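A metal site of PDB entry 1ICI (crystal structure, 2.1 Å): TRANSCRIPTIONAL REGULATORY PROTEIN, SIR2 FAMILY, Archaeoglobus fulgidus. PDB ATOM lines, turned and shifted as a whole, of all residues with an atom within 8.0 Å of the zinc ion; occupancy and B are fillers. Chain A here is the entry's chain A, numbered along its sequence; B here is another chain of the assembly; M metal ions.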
ATOM      1  N   ARG A 134     -23.762  25.134 -17.456  1.00  0.00           N
ATOM      2  CA  ARG A 134     -23.581  25.135 -16.007  1.00  0.00           C
ATOM      3  C   ARG A 134     -22.370  24.318 -15.579  1.00  0.00           C
ATOM      4  O   ARG A 134     -21.874  23.474 -16.325  1.00  0.00           O
ATOM      5  CB  ARG A 134     -24.827  24.607 -15.300  1.00  0.00           C
ATOM      6  CG  ARG A 134     -25.104  23.124 -15.451  1.00  0.00           C
ATOM      7  CD  ARG A 134     -26.356  22.783 -14.671  1.00  0.00           C
ATOM      8  NE  ARG A 134     -26.654  21.352 -14.641  1.00  0.00           N
ATOM      9  CZ  ARG A 134     -25.925  20.451 -13.985  1.00  0.00           C
ATOM     10  NH1 ARG A 134     -24.859  20.831 -13.300  1.00  0.00           N
ATOM     11  NH2 ARG A 134     -26.289  19.172 -14.012  1.00  0.00           N
ATOM     12  N   CYS A 135     -21.877  24.574 -14.376  1.00  0.00           N
ATOM     13  CA  CYS A 135     -20.703  23.875 -13.883  1.00  0.00           C
ATOM     14  C   CYS A 135     -21.015  22.471 -13.387  1.00  0.00           C
ATOM     15  O   CYS A 135     -22.083  22.232 -12.827  1.00  0.00           O
ATOM     16  CB  CYS A 135     -20.028  24.670 -12.746  1.00  0.00           C
ATOM     17  SG  CYS A 135     -18.521  23.874 -12.146  1.00  0.00           S
ATOM     18  N   THR A 136     -20.068  21.560 -13.604  1.00  0.00           N
ATOM     19  CA  THR A 136     -20.199  20.180 -13.150  1.00  0.00           C
ATOM     20  C   THR A 136     -19.882  20.091 -11.673  1.00  0.00           C
ATOM     21  O   THR A 136     -20.185  19.079 -11.040  1.00  0.00           O
ATOM     22  CB  THR A 136     -19.182  19.248 -13.846  1.00  0.00           C
ATOM     23  OG1 THR A 136     -17.856  19.725 -13.574  1.00  0.00           O
ATOM     24  CG2 THR A 136     -19.426  19.178 -15.360  1.00  0.00           C
ATOM     25  N   SER A 137     -19.262  21.133 -11.120  1.00  0.00           N
ATOM     26  CA  SER A 137     -18.824  21.094  -9.726  1.00  0.00           C
ATOM     27  C   SER A 137     -19.499  22.045  -8.750  1.00  0.00           C
ATOM     28  O   SER A 137     -19.929  21.606  -7.676  1.00  0.00           O
ATOM     29  CB  SER A 137     -17.308  21.304  -9.706  1.00  0.00           C
ATOM     30  OG  SER A 137     -16.752  20.919  -8.467  1.00  0.00           O
ATOM     31  N   CYS A 138     -19.573  23.332  -9.072  1.00  0.00           N
ATOM     32  CA  CYS A 138     -20.236  24.307  -8.212  1.00  0.00           C
ATOM     33  C   CYS A 138     -21.604  24.630  -8.842  1.00  0.00           C
ATOM     34  O   CYS A 138     -21.982  24.008  -9.839  1.00  0.00           O
ATOM     35  CB  CYS A 138     -19.378  25.570  -8.034  1.00  0.00           C
ATOM     36  SG  CYS A 138     -19.249  26.683  -9.476  1.00  0.00           S
ATOM     37  N   ASN A 139     -22.353  25.579  -8.259  1.00  0.00           N
ATOM     38  CA  ASN A 139     -23.677  25.934  -8.774  1.00  0.00           C
ATOM     39  C   ASN A 139     -23.714  26.995  -9.877  1.00  0.00           C
ATOM     40  O   ASN A 139     -24.797  27.417 -10.311  1.00  0.00           O
ATOM     41  CB  ASN A 139     -24.589  26.408  -7.638  1.00  0.00           C
ATOM     42  CG  ASN A 139     -24.842  25.334  -6.615  1.00  0.00           C
ATOM     43  OD1 ASN A 139     -25.213  24.215  -6.963  1.00  0.00           O
ATOM     44  ND2 ASN A 139     -24.641  25.659  -5.353  1.00  0.00           N
ATOM     45  N   ASN A 140     -22.556  27.440 -10.321  1.00  0.00           N
ATOM     46  CA  ASN A 140     -22.476  28.445 -11.359  1.00  0.00           C
ATOM     47  C   ASN A 140     -23.320  28.026 -12.577  1.00  0.00           C
ATOM     48  O   ASN A 140     -23.212  26.896 -13.049  1.00  0.00           O
ATOM     49  CB  ASN A 140     -21.004  28.645 -11.727  1.00  0.00           C
ATOM     50  CG  ASN A 140     -20.807  29.754 -12.739  1.00  0.00           C
ATOM     51  OD1 ASN A 140     -21.505  30.757 -12.728  1.00  0.00           O
ATOM     52  ND2 ASN A 140     -19.828  29.564 -13.624  1.00  0.00           N
ATOM     53  N   SER A 141     -24.179  28.924 -13.058  1.00  0.00           N
ATOM     54  CA  SER A 141     -25.037  28.653 -14.213  1.00  0.00           C
ATOM     55  C   SER A 141     -25.294  29.958 -14.988  1.00  0.00           C
ATOM     56  O   SER A 141     -25.458  31.022 -14.395  1.00  0.00           O
ATOM     57  CB  SER A 141     -26.367  28.046 -13.751  1.00  0.00           C
ATOM     58  OG  SER A 141     -27.062  27.491 -14.846  1.00  0.00           O
ATOM     59  N   LYS A 155     -14.361  25.876 -19.066  1.00  0.00           N
ATOM     60  CA  LYS A 155     -14.106  25.728 -17.645  1.00  0.00           C
ATOM     61  C   LYS A 155     -14.749  26.847 -16.841  1.00  0.00           C
ATOM     62  O   LYS A 155     -14.733  28.001 -17.259  1.00  0.00           O
ATOM     63  CB  LYS A 155     -12.598  25.716 -17.392  1.00  0.00           C
ATOM     64  CG  LYS A 155     -11.870  24.682 -18.228  1.00  0.00           C
ATOM     65  CD  LYS A 155     -11.161  23.658 -17.355  1.00  0.00           C
ATOM     66  CE  LYS A 155     -10.571  22.567 -18.213  1.00  0.00           C
ATOM     67  NZ  LYS A 155      -9.754  21.628 -17.416  1.00  0.00           N
ATOM     68  N   CYS A 156     -15.314  26.488 -15.694  1.00  0.00           N
ATOM     69  CA  CYS A 156     -15.996  27.430 -14.810  1.00  0.00           C
ATOM     70  C   CYS A 156     -15.057  28.523 -14.268  1.00  0.00           C
ATOM     71  O   CYS A 156     -13.980  28.216 -13.747  1.00  0.00           O
ATOM     72  CB  CYS A 156     -16.595  26.643 -13.651  1.00  0.00           C
ATOM     73  SG  CYS A 156     -17.429  27.625 -12.421  1.00  0.00           S
ATOM     74  N   ASP A 157     -15.463  29.785 -14.383  1.00  0.00           N
ATOM     75  CA  ASP A 157     -14.619  30.876 -13.880  1.00  0.00           C
ATOM     76  C   ASP A 157     -14.791  31.124 -12.375  1.00  0.00           C
ATOM     77  O   ASP A 157     -14.245  32.089 -11.838  1.00  0.00           O
ATOM     78  CB  ASP A 157     -14.849  32.184 -14.681  1.00  0.00           C
ATOM     79  CG  ASP A 157     -16.274  32.705 -14.599  1.00  0.00           C
ATOM     80  OD1 ASP A 157     -16.622  33.555 -15.441  1.00  0.00           O
ATOM     81  OD2 ASP A 157     -17.050  32.290 -13.708  1.00  0.00           O
ATOM     82  N   LYS A 158     -15.543  30.243 -11.711  1.00  0.00           N
ATOM     83  CA  LYS A 158     -15.742  30.347 -10.250  1.00  0.00           C
ATOM     84  C   LYS A 158     -14.932  29.274  -9.518  1.00  0.00           C
ATOM     85  O   LYS A 158     -14.282  29.563  -8.502  1.00  0.00           O
ATOM     86  CB  LYS A 158     -17.220  30.194  -9.878  1.00  0.00           C
ATOM     87  CG  LYS A 158     -18.148  31.208 -10.550  1.00  0.00           C
ATOM     88  CD  LYS A 158     -17.792  32.645 -10.209  1.00  0.00           C
ATOM     89  CE  LYS A 158     -18.653  33.598 -11.016  1.00  0.00           C
ATOM     90  NZ  LYS A 158     -18.201  34.998 -10.888  1.00  0.00           N
ATOM     91  N   CYS A 159     -14.970  28.030 -10.023  1.00  0.00           N
ATOM     92  CA  CYS A 159     -14.250  26.936  -9.362  1.00  0.00           C
ATOM     93  C   CYS A 159     -13.229  26.222 -10.236  1.00  0.00           C
ATOM     94  O   CYS A 159     -12.603  25.251  -9.801  1.00  0.00           O
ATOM     95  CB  CYS A 159     -15.249  25.904  -8.835  1.00  0.00           C
ATOM     96  SG  CYS A 159     -15.946  24.848 -10.119  1.00  0.00           S
ATOM     97  N   GLY A 160     -13.066  26.701 -11.466  1.00  0.00           N
ATOM     98  CA  GLY A 160     -12.118  26.102 -12.389  1.00  0.00           C
ATOM     99  C   GLY A 160     -12.526  24.760 -12.972  1.00  0.00           C
ATOM    100  O   GLY A 160     -11.828  24.230 -13.840  1.00  0.00           O
ATOM    101  N   SER A 161     -13.659  24.212 -12.547  1.00  0.00           N
ATOM    102  CA  SER A 161     -14.075  22.907 -13.064  1.00  0.00           C
ATOM    103  C   SER A 161     -14.699  22.911 -14.467  1.00  0.00           C
ATOM    104  O   SER A 161     -14.915  23.945 -15.105  1.00  0.00           O
ATOM    105  CB  SER A 161     -15.039  22.240 -12.074  1.00  0.00           C
ATOM    106  OG  SER A 161     -14.487  22.215 -10.773  1.00  0.00           O
ATOM    107  N   LEU A 162     -14.983  21.711 -14.943  1.00  0.00           N
ATOM    108  CA  LEU A 162     -15.554  21.535 -16.260  1.00  0.00           C
ATOM    109  C   LEU A 162     -17.004  22.009 -16.310  1.00  0.00           C
ATOM    110  O   LEU A 162     -17.784  21.732 -15.407  1.00  0.00           O
ATOM    111  CB  LEU A 162     -15.479  20.054 -16.628  1.00  0.00           C
ATOM    112  CG  LEU A 162     -15.555  19.636 -18.089  1.00  0.00           C
ATOM    113  CD1 LEU A 162     -14.493  20.362 -18.927  1.00  0.00           C
ATOM    114  CD2 LEU A 162     -15.330  18.134 -18.147  1.00  0.00           C
ATOM    115  N   LEU A 163     -17.324  22.777 -17.334  1.00  0.00           N
ATOM    116  CA  LEU A 163     -18.706  23.217 -17.506  1.00  0.00           C
ATOM    117  C   LEU A 163     -19.371  22.134 -18.366  1.00  0.00           C
ATOM    118  O   LEU A 163     -18.688  21.338 -19.005  1.00  0.00           O
ATOM    119  CB  LEU A 163     -18.760  24.561 -18.239  1.00  0.00           C
ATOM    120  CG  LEU A 163     -18.304  25.799 -17.467  1.00  0.00           C
ATOM    121  CD1 LEU A 163     -18.131  26.972 -18.441  1.00  0.00           C
ATOM    122  CD2 LEU A 163     -19.331  26.148 -16.406  1.00  0.00           C
ATOM    123  N   PRO B 176     -13.424  29.916  -5.411  1.00  0.00           N
ATOM    124  CA  PRO B 176     -12.143  29.238  -5.301  1.00  0.00           C
ATOM    125  C   PRO B 176     -11.161  29.487  -6.426  1.00  0.00           C
ATOM    126  O   PRO B 176      -9.980  29.772  -6.169  1.00  0.00           O
ATOM    127  CB  PRO B 176     -12.528  27.760  -5.186  1.00  0.00           C
ATOM    128  CG  PRO B 176     -13.902  27.783  -4.599  1.00  0.00           C
ATOM    129  CD  PRO B 176     -14.536  28.931  -5.353  1.00  0.00           C
ATOM    130  N   ASP B 177     -11.618  29.394  -7.667  1.00  0.00           N
ATOM    131  CA  ASP B 177     -10.708  29.587  -8.789  1.00  0.00           C
ATOM    132  C   ASP B 177     -10.193  31.023  -8.783  1.00  0.00           C
ATOM    133  O   ASP B 177      -9.052  31.282  -9.130  1.00  0.00           O
ATOM    134  CB  ASP B 177     -11.430  29.268 -10.099  1.00  0.00           C
ATOM    135  CG  ASP B 177     -10.498  29.283 -11.286  1.00  0.00           C
ATOM    136  OD1 ASP B 177      -9.549  28.472 -11.303  1.00  0.00           O
ATOM    137  OD2 ASP B 177     -10.716  30.109 -12.187  1.00  0.00           O
HETATM  138 ZN    ZN M   1     -17.791  25.859 -10.924  1.00  0.00          ZN
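The side-chain amide nitrogen of Asn 140 lies close to the side-chain sulfur of Cys 156 (3.3 Å). The backbone NH of Cys 156 lies within hydrogen-bond range of the backbone carbonyl oxygen of Ser 161. N of Asn 140 sits close to SG of Cys 138, at 3.5 Å. The backbone NH of Lys 158 sits close to the side-chain sulfur of Cys 156, at 3.3 Å. SG of Cys 135 lies close to N of Ser 137. N of Cys 135 sits at hydrogen-bond distance from O of Asn 140. OG of Ser 161 sits close to SG of Cys 159 (3.1 Å).
The zinc ion is bound by SG of Cys 138, SG of Cys 159, SG of Cys 156 and SG of Cys 135. The zinc ion has four donor atoms within binding distance.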
